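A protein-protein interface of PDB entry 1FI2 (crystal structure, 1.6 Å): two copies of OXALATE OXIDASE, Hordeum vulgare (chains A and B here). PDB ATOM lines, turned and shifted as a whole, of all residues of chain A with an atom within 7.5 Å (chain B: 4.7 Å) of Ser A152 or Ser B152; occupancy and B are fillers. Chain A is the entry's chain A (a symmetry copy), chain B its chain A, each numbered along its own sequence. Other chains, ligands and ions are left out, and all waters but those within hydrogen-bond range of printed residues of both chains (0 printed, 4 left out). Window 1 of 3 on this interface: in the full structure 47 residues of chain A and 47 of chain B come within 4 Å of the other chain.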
ATOM      1  N   VAL A  72       6.646 -17.463   2.749  1.00  0.00           N
ATOM      2  CA  VAL A  72       5.428 -16.813   2.305  1.00  0.00           C
ATOM      3  C   VAL A  72       4.624 -16.259   3.486  1.00  0.00           C
ATOM      4  O   VAL A  72       4.851 -16.598   4.644  1.00  0.00           O
ATOM      5  CB  VAL A  72       4.470 -17.743   1.532  1.00  0.00           C
ATOM      6  CG1 VAL A  72       4.950 -18.118   0.138  1.00  0.00           C
ATOM      7  CG2 VAL A  72       4.208 -19.008   2.349  1.00  0.00           C
ATOM      8  N   SER A  73       3.733 -15.327   3.161  1.00  0.00           N
ATOM      9  CA  SER A  73       2.809 -14.749   4.129  1.00  0.00           C
ATOM     10  C   SER A  73       1.739 -13.955   3.381  1.00  0.00           C
ATOM     11  O   SER A  73       1.830 -13.802   2.162  1.00  0.00           O
ATOM     12  CB  SER A  73       3.518 -13.874   5.154  1.00  0.00           C
ATOM     13  OG  SER A  73       3.968 -12.663   4.575  1.00  0.00           O
ATOM     14  N   MET A  74       0.686 -13.529   4.077  1.00  0.00           N
ATOM     15  CA  MET A  74      -0.395 -12.787   3.451  1.00  0.00           C
ATOM     16  C   MET A  74      -0.857 -11.623   4.328  1.00  0.00           C
ATOM     17  O   MET A  74      -0.433 -11.442   5.463  1.00  0.00           O
ATOM     18  CB  MET A  74      -1.642 -13.657   3.249  1.00  0.00           C
ATOM     19  CG  MET A  74      -1.553 -14.779   2.241  1.00  0.00           C
ATOM     20  SD  MET A  74      -2.958 -15.901   2.362  1.00  0.00           S
ATOM     21  CE  MET A  74      -4.120 -15.129   1.263  1.00  0.00           C
ATOM     22  N   ASN A  75      -1.796 -10.851   3.783  1.00  0.00           N
ATOM     23  CA  ASN A  75      -2.527  -9.875   4.586  1.00  0.00           C
ATOM     24  C   ASN A  75      -3.793  -9.462   3.838  1.00  0.00           C
ATOM     25  O   ASN A  75      -3.908  -9.689   2.637  1.00  0.00           O
ATOM     26  CB  ASN A  75      -1.693  -8.693   5.007  1.00  0.00           C
ATOM     27  CG  ASN A  75      -1.350  -7.583   4.067  1.00  0.00           C
ATOM     28  OD1 ASN A  75      -0.298  -6.940   4.252  1.00  0.00           O
ATOM     29  ND2 ASN A  75      -2.165  -7.279   3.066  1.00  0.00           N
ATOM     30  N   ALA A  93      10.412  -8.079   0.329  1.00  0.00           N
ATOM     31  CA  ALA A  93       9.566  -8.935  -0.493  1.00  0.00           C
ATOM     32  C   ALA A  93       8.818  -8.260  -1.634  1.00  0.00           C
ATOM     33  O   ALA A  93       8.467  -7.091  -1.593  1.00  0.00           O
ATOM     34  CB  ALA A  93       8.500  -9.586   0.401  1.00  0.00           C
ATOM     35  N   THR A  94       8.461  -9.108  -2.597  1.00  0.00           N
ATOM     36  CA  THR A  94       7.549  -8.783  -3.684  1.00  0.00           C
ATOM     37  C   THR A  94       6.131  -9.077  -3.191  1.00  0.00           C
ATOM     38  O   THR A  94       5.930 -10.028  -2.436  1.00  0.00           O
ATOM     39  CB  THR A  94       7.822  -9.643  -4.932  1.00  0.00           C
ATOM     40  OG1 THR A  94       9.117  -9.349  -5.481  1.00  0.00           O
ATOM     41  CG2 THR A  94       6.777  -9.415  -6.021  1.00  0.00           C
ATOM     42  N   GLU A  95       5.164  -8.275  -3.603  1.00  0.00           N
ATOM     43  CA  GLU A  95       3.767  -8.474  -3.230  1.00  0.00           C
ATOM     44  C   GLU A  95       2.942  -8.810  -4.470  1.00  0.00           C
ATOM     45  O   GLU A  95       3.151  -8.253  -5.548  1.00  0.00           O
ATOM     46  CB  GLU A  95       3.219  -7.224  -2.543  1.00  0.00           C
ATOM     47  CG  GLU A  95       1.728  -7.179  -2.274  1.00  0.00           C
ATOM     48  CD  GLU A  95       1.255  -5.827  -1.781  1.00  0.00           C
ATOM     49  OE1 GLU A  95       2.112  -4.976  -1.467  1.00  0.00           O
ATOM     50  OE2 GLU A  95       0.035  -5.580  -1.708  1.00  0.00           O
ATOM     51  N   ILE A  96       2.012  -9.741  -4.300  1.00  0.00           N
ATOM     52  CA  ILE A  96       1.115 -10.148  -5.389  1.00  0.00           C
ATOM     53  C   ILE A  96      -0.296 -10.194  -4.822  1.00  0.00           C
ATOM     54  O   ILE A  96      -0.540 -10.871  -3.820  1.00  0.00           O
ATOM     55  CB  ILE A  96       1.602 -11.444  -6.041  1.00  0.00           C
ATOM     56  CG1 ILE A  96       0.805 -11.763  -7.310  1.00  0.00           C
ATOM     57  CG2 ILE A  96       1.579 -12.624  -5.078  1.00  0.00           C
ATOM     58  CD1 ILE A  96       1.456 -12.823  -8.180  1.00  0.00           C
ATOM     59  N   GLY A  97      -1.215  -9.391  -5.376  1.00  0.00           N
ATOM     60  CA  GLY A  97      -2.538  -9.318  -4.766  1.00  0.00           C
ATOM     61  C   GLY A  97      -3.722  -9.394  -5.705  1.00  0.00           C
ATOM     62  O   GLY A  97      -3.600  -9.307  -6.924  1.00  0.00           O
ATOM     63  N   MET A  98      -4.897  -9.576  -5.102  1.00  0.00           N
ATOM     64  CA  MET A  98      -6.145  -9.648  -5.847  1.00  0.00           C
ATOM     65  C   MET A  98      -7.191  -8.768  -5.160  1.00  0.00           C
ATOM     66  O   MET A  98      -7.331  -8.843  -3.941  1.00  0.00           O
ATOM     67  CB  MET A  98      -6.675 -11.081  -5.981  1.00  0.00           C
ATOM     68  CG  MET A  98      -7.964 -11.126  -6.797  1.00  0.00           C
ATOM     69  SD  MET A  98      -8.713 -12.759  -6.904  1.00  0.00           S
ATOM     70  CE  MET A  98      -7.766 -13.476  -8.240  1.00  0.00           C
ATOM     71  N   PHE A 129      -2.585  -7.607  -9.277  1.00  0.00           N
ATOM     72  CA  PHE A 129      -1.473  -6.683  -9.420  1.00  0.00           C
ATOM     73  C   PHE A 129      -0.204  -7.252  -8.783  1.00  0.00           C
ATOM     74  O   PHE A 129      -0.269  -8.124  -7.917  1.00  0.00           O
ATOM     75  CB  PHE A 129      -1.791  -5.333  -8.773  1.00  0.00           C
ATOM     76  CG  PHE A 129      -2.114  -5.356  -7.307  1.00  0.00           C
ATOM     77  CD1 PHE A 129      -1.118  -5.304  -6.347  1.00  0.00           C
ATOM     78  CD2 PHE A 129      -3.432  -5.414  -6.880  1.00  0.00           C
ATOM     79  CE1 PHE A 129      -1.425  -5.320  -5.002  1.00  0.00           C
ATOM     80  CE2 PHE A 129      -3.752  -5.430  -5.534  1.00  0.00           C
ATOM     81  CZ  PHE A 129      -2.741  -5.386  -4.594  1.00  0.00           C
ATOM     82  N   ILE A 131       3.713  -6.017  -7.137  1.00  0.00           N
ATOM     83  CA  ILE A 131       4.592  -4.942  -6.697  1.00  0.00           C
ATOM     84  C   ILE A 131       6.008  -5.476  -6.482  1.00  0.00           C
ATOM     85  O   ILE A 131       6.252  -6.174  -5.497  1.00  0.00           O
ATOM     86  CB  ILE A 131       4.177  -4.378  -5.318  1.00  0.00           C
ATOM     87  CG1 ILE A 131       2.678  -4.169  -5.153  1.00  0.00           C
ATOM     88  CG2 ILE A 131       4.961  -3.102  -5.032  1.00  0.00           C
ATOM     89  CD1 ILE A 131       2.061  -3.026  -5.909  1.00  0.00           C
ATOM     90  N   VAL A 150      -6.863  -9.042  -0.869  1.00  0.00           N
ATOM     91  CA  VAL A 150      -6.031 -10.002  -0.153  1.00  0.00           C
ATOM     92  C   VAL A 150      -4.740 -10.166  -0.957  1.00  0.00           C
ATOM     93  O   VAL A 150      -4.820 -10.393  -2.168  1.00  0.00           O
ATOM     94  CB  VAL A 150      -6.718 -11.362   0.036  1.00  0.00           C
ATOM     95  CG1 VAL A 150      -5.768 -12.354   0.696  1.00  0.00           C
ATOM     96  CG2 VAL A 150      -7.992 -11.253   0.866  1.00  0.00           C
ATOM     97  N   VAL A 151      -3.587  -9.982  -0.321  1.00  0.00           N
ATOM     98  CA  VAL A 151      -2.309 -10.082  -1.009  1.00  0.00           C
ATOM     99  C   VAL A 151      -1.410 -11.142  -0.373  1.00  0.00           C
ATOM    100  O   VAL A 151      -1.559 -11.495   0.796  1.00  0.00           O
ATOM    101  CB  VAL A 151      -1.553  -8.741  -1.047  1.00  0.00           C
ATOM    102  CG1 VAL A 151      -2.423  -7.581  -1.520  1.00  0.00           C
ATOM    103  CG2 VAL A 151      -0.950  -8.402   0.310  1.00  0.00           C
ATOM    104  N   SER A 152      -0.434 -11.602  -1.149  1.00  0.00           N
ATOM    105  CA  SER A 152       0.557 -12.558  -0.686  1.00  0.00           C
ATOM    106  C   SER A 152       1.941 -11.943  -0.896  1.00  0.00           C
ATOM    107  O   SER A 152       2.103 -11.042  -1.715  1.00  0.00           O
ATOM    108  CB  SER A 152       0.475 -13.891  -1.419  1.00  0.00           C
ATOM    109  OG  SER A 152      -0.771 -14.529  -1.214  1.00  0.00           O
ATOM    110  N   PHE A 153       2.903 -12.415  -0.117  1.00  0.00           N
ATOM    111  CA  PHE A 153       4.267 -11.929  -0.193  1.00  0.00           C
ATOM    112  C   PHE A 153       5.223 -13.119  -0.296  1.00  0.00           C
ATOM    113  O   PHE A 153       4.930 -14.205   0.199  1.00  0.00           O
ATOM    114  CB  PHE A 153       4.691 -11.129   1.040  1.00  0.00           C
ATOM    115  CG  PHE A 153       3.856  -9.916   1.332  1.00  0.00           C
ATOM    116  CD1 PHE A 153       2.741 -10.012   2.146  1.00  0.00           C
ATOM    117  CD2 PHE A 153       4.186  -8.684   0.788  1.00  0.00           C
ATOM    118  CE1 PHE A 153       1.962  -8.902   2.412  1.00  0.00           C
ATOM    119  CE2 PHE A 153       3.410  -7.571   1.050  1.00  0.00           C
ATOM    120  CZ  PHE A 153       2.302  -7.676   1.865  1.00  0.00           C
ATOM    121  N   ASN A 154       6.428 -12.825  -0.769  1.00  0.00           N
ATOM    122  CA  ASN A 154       7.440 -13.877  -0.874  1.00  0.00           C
ATOM    123  C   ASN A 154       8.443 -13.798   0.272  1.00  0.00           C
ATOM    124  O   ASN A 154       9.630 -14.046   0.129  1.00  0.00           O
ATOM    125  CB  ASN A 154       8.094 -13.869  -2.232  1.00  0.00           C
ATOM    126  CG  ASN A 154       9.003 -12.770  -2.672  1.00  0.00           C
ATOM    127  OD1 ASN A 154       8.837 -11.619  -2.308  1.00  0.00           O
ATOM    128  ND2 ASN A 154       9.976 -13.174  -3.494  1.00  0.00           N
ATOM    129  N   SER A 155       7.902 -13.548   1.451  1.00  0.00           N
ATOM    130  CA  SER A 155       8.623 -13.502   2.699  1.00  0.00           C
ATOM    131  C   SER A 155       7.639 -13.783   3.836  1.00  0.00           C
ATOM    132  O   SER A 155       6.458 -13.441   3.753  1.00  0.00           O
ATOM    133  CB  SER A 155       9.289 -12.146   2.955  1.00  0.00           C
ATOM    134  OG  SER A 155       9.924 -12.172   4.231  1.00  0.00           O
ATOM    135  N   PRO A 158       7.661  -9.548   5.434  1.00  0.00           N
ATOM    136  CA  PRO A 158       8.004  -8.553   4.443  1.00  0.00           C
ATOM    137  C   PRO A 158       8.464  -7.219   5.005  1.00  0.00           C
ATOM    138  O   PRO A 158       9.345  -6.575   4.426  1.00  0.00           O
ATOM    139  CB  PRO A 158       6.746  -8.385   3.596  1.00  0.00           C
ATOM    140  CG  PRO A 158       5.643  -9.040   4.337  1.00  0.00           C
ATOM    141  CD  PRO A 158       6.266 -10.030   5.281  1.00  0.00           C
ATOM    142  N   SER B  73       3.801 -15.790  -8.374  1.00  0.00           N
ATOM    143  CA  SER B  73       2.777 -16.103  -9.365  1.00  0.00           C
ATOM    144  C   SER B  73       1.518 -16.580  -8.643  1.00  0.00           C
ATOM    145  O   SER B  73       1.537 -16.748  -7.422  1.00  0.00           O
ATOM    146  CB  SER B  73       3.249 -17.139 -10.376  1.00  0.00           C
ATOM    147  OG  SER B  73       3.346 -18.424  -9.791  1.00  0.00           O
ATOM    148  N   MET B  74       0.405 -16.711  -9.363  1.00  0.00           N
ATOM    149  CA  MET B  74      -0.849 -17.134  -8.764  1.00  0.00           C
ATOM    150  C   MET B  74      -1.586 -18.134  -9.654  1.00  0.00           C
ATOM    151  O   MET B  74      -1.200 -18.426 -10.781  1.00  0.00           O
ATOM    152  CB  MET B  74      -1.822 -15.961  -8.587  1.00  0.00           C
ATOM    153  CG  MET B  74      -1.459 -14.901  -7.574  1.00  0.00           C
ATOM    154  SD  MET B  74      -2.509 -13.445  -7.723  1.00  0.00           S
ATOM    155  CE  MET B  74      -3.860 -13.875  -6.653  1.00  0.00           C
ATOM    156  N   THR B  94       6.564 -23.029  -2.531  1.00  0.00           N
ATOM    157  CA  THR B  94       5.575 -23.095  -1.466  1.00  0.00           C
ATOM    158  C   THR B  94       4.298 -22.434  -1.990  1.00  0.00           C
ATOM    159  O   THR B  94       4.376 -21.467  -2.745  1.00  0.00           O
ATOM    160  CB  THR B  94       6.039 -22.335  -0.209  1.00  0.00           C
ATOM    161  OG1 THR B  94       7.196 -22.964   0.368  1.00  0.00           O
ATOM    162  CG2 THR B  94       4.948 -22.273   0.855  1.00  0.00           C
ATOM    163  N   GLU B  95       3.143 -22.947  -1.601  1.00  0.00           N
ATOM    164  CA  GLU B  95       1.858 -22.383  -2.005  1.00  0.00           C
ATOM    165  C   GLU B  95       1.126 -21.835  -0.783  1.00  0.00           C
ATOM    166  O   GLU B  95       1.155 -22.425   0.298  1.00  0.00           O
ATOM    167  CB  GLU B  95       1.012 -23.442  -2.708  1.00  0.00           C
ATOM    168  CG  GLU B  95      -0.430 -23.088  -3.010  1.00  0.00           C
ATOM    169  CD  GLU B  95      -1.237 -24.266  -3.518  1.00  0.00           C
ATOM    170  OE1 GLU B  95      -0.632 -25.316  -3.815  1.00  0.00           O
ATOM    171  OE2 GLU B  95      -2.477 -24.178  -3.618  1.00  0.00           O
ATOM    172  N   ILE B  96       0.483 -20.690  -0.970  1.00  0.00           N
ATOM    173  CA  ILE B  96      -0.297 -20.054   0.100  1.00  0.00           C
ATOM    174  C   ILE B  96      -1.632 -19.634  -0.499  1.00  0.00           C
ATOM    175  O   ILE B  96      -1.663 -18.920  -1.503  1.00  0.00           O
ATOM    176  CB  ILE B  96       0.504 -18.933   0.766  1.00  0.00           C
ATOM    177  CG1 ILE B  96      -0.206 -18.409   2.018  1.00  0.00           C
ATOM    178  CG2 ILE B  96       0.819 -17.793  -0.193  1.00  0.00           C
ATOM    179  CD1 ILE B  96       0.685 -17.559   2.906  1.00  0.00           C
ATOM    180  N   VAL B 150      -8.177 -19.000  -4.600  1.00  0.00           N
ATOM    181  CA  VAL B 150      -7.103 -18.299  -5.295  1.00  0.00           C
ATOM    182  C   VAL B 150      -5.833 -18.484  -4.461  1.00  0.00           C
ATOM    183  O   VAL B 150      -5.877 -18.241  -3.252  1.00  0.00           O
ATOM    184  CB  VAL B 150      -7.397 -16.806  -5.495  1.00  0.00           C
ATOM    185  CG1 VAL B 150      -6.201 -16.106  -6.130  1.00  0.00           C
ATOM    186  CG2 VAL B 150      -8.635 -16.572  -6.354  1.00  0.00           C
ATOM    187  N   VAL B 151      -4.758 -18.972  -5.073  1.00  0.00           N
ATOM    188  CA  VAL B 151      -3.515 -19.215  -4.356  1.00  0.00           C
ATOM    189  C   VAL B 151      -2.351 -18.436  -4.968  1.00  0.00           C
ATOM    190  O   VAL B 151      -2.374 -18.059  -6.139  1.00  0.00           O
ATOM    191  CB  VAL B 151      -3.147 -20.709  -4.305  1.00  0.00           C
ATOM    192  CG1 VAL B 151      -4.305 -21.593  -3.855  1.00  0.00           C
ATOM    193  CG2 VAL B 151      -2.626 -21.202  -5.650  1.00  0.00           C
ATOM    194  N   SER B 152      -1.306 -18.252  -4.170  1.00  0.00           N
ATOM    195  CA  SER B 152      -0.085 -17.597  -4.607  1.00  0.00           C
ATOM    196  C   SER B 152       1.079 -18.559  -4.369  1.00  0.00           C
ATOM    197  O   SER B 152       0.976 -19.468  -3.549  1.00  0.00           O
ATOM    198  CB  SER B 152       0.177 -16.289  -3.872  1.00  0.00           C
ATOM    199  OG  SER B 152      -0.848 -15.341  -4.103  1.00  0.00           O
ATOM    200  N   PHE B 153       2.150 -18.364  -5.125  1.00  0.00           N
ATOM    201  CA  PHE B 153       3.332 -19.196  -5.020  1.00  0.00           C
ATOM    202  C   PHE B 153       4.568 -18.305  -4.892  1.00  0.00           C
ATOM    203  O   PHE B 153       4.588 -17.182  -5.390  1.00  0.00           O
ATOM    204  CB  PHE B 153       3.554 -20.085  -6.245  1.00  0.00           C
ATOM    205  CG  PHE B 153       2.431 -21.031  -6.560  1.00  0.00           C
ATOM    206  CD1 PHE B 153       1.401 -20.642  -7.398  1.00  0.00           C
ATOM    207  CD2 PHE B 153       2.408 -22.305  -6.012  1.00  0.00           C
ATOM    208  CE1 PHE B 153       0.360 -21.505  -7.684  1.00  0.00           C
ATOM    209  CE2 PHE B 153       1.368 -23.170  -6.294  1.00  0.00           C
ATOM    210  CZ  PHE B 153       0.347 -22.776  -7.134  1.00  0.00           C
ATOM    211  N   ASN B 154       5.640 -18.910  -4.393  1.00  0.00           N
ATOM    212  CA  ASN B 154       6.894 -18.167  -4.262  1.00  0.00           C
ATOM    213  C   ASN B 154       7.865 -18.514  -5.385  1.00  0.00           C
ATOM    214  O   ASN B 154       9.072 -18.593  -5.216  1.00  0.00           O
ATOM    215  CB  ASN B 154       7.491 -18.344  -2.889  1.00  0.00           C
ATOM    216  CG  ASN B 154       8.064 -19.646  -2.434  1.00  0.00           C
ATOM    217  OD1 ASN B 154       7.604 -20.711  -2.804  1.00  0.00           O
ATOM    218  ND2 ASN B 154       9.091 -19.514  -1.589  1.00  0.00           N
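Printed residues of chain B that touch a printed residue of chain A: Ser B73, Met B74, Thr B94, Ile B96, Val B150, Ser B152 and Asn B154. Among the printed residues, no Asp or Glu carboxylate lies within 4 Å of a Lys or Arg side-chain nitrogen of the other chain.
OG of Ser A152 is in hydrogen-bond range of OG of Ser B152, at 3.0 Å.
The backbone carbonyl oxygen of Ser A73 is in hydrogen-bond range of the backbone NH of Phe A153. The backbone carbonyl oxygen of Ile A96 is in hydrogen-bond range of the backbone NH of Ser A152 (2.8 Å). The backbone carbonyl oxygen (O) of Ser B73 sits at hydrogen-bond distance from the backbone NH (N) of Phe B153, at 2.9 Å. The backbone carbonyl oxygen of Ile B96 lies within hydrogen-bond range of the backbone NH of Ser B152. The backbone carbonyl oxygen (O) of Ser A155 sits at hydrogen-bond distance from the side-chain hydroxyl (OG) of Ser A73, at 2.7 Å. The backbone NH (N) of Met A98 lies within hydrogen-bond range of the backbone carbonyl oxygen (O) of Val A150 (3.0 Å).
Of the printed residues of chain B, Ser A73 touches Ile B96 (3.7 Å). Printed residues of chain B within 4 Å of Met A98: Val B150. Of chain B, only Ile B96 (3.8 Å) and Ser B152 (3.0 Å) come within 4 Å of Ser A152. Of the printed residues of chain A, Thr B94 touches Val A72 (3.7 Å). Of the printed residues of chain A, Ile B96 touches Val A72, Ser A73, Met A74 and Ser A152. The nearest residue of chain A that does not touch Ser B152 is Val A72 (5.6 Å). The nearest printed residue of chain A that does not touch Val B150 is Met A74 (5.8 Å).
Ser A73 touches Ile B96, and with the chains exchanged Ile A96 touches Ser B73. Met A74 touches Ile B96, and with the chains exchanged Ile A96 touches Met B74. Ile A96 touches Ser B152, and with the chains exchanged Ser A152 touches Ile B96. Ser B152 touches its own counterpart, Ser A152. 10 positions are printed for both chains. Of the 11 pairs that touch across the chains among the printed residues, 7 have their exchanged pair printed and touching as well.
CG2 of Val A72 touches CG2 of Thr B94, 3.7 Å away. Val A72 touches Ile B96 (CG2 to CD1, 3.8 Å). CG1 of Val A72 touches CB of Asn B154 (3.96 Å). Ile B96 touches Ser A73 (CD1 to CA, 3.7 Å). Ile B96 touches Met A74. Ser B73 touches Ile A96 (CA to CD1, 3.7 Å). CD1 of Ile A96 touches CG of Met B74 (3.6 Å). OG of Ser B152 touches CG2 of Ile A96 (3.8 Å). Met A98 touches Val B150. CG2 of Ile B96 touches OG of Ser A152 (3.8 Å).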
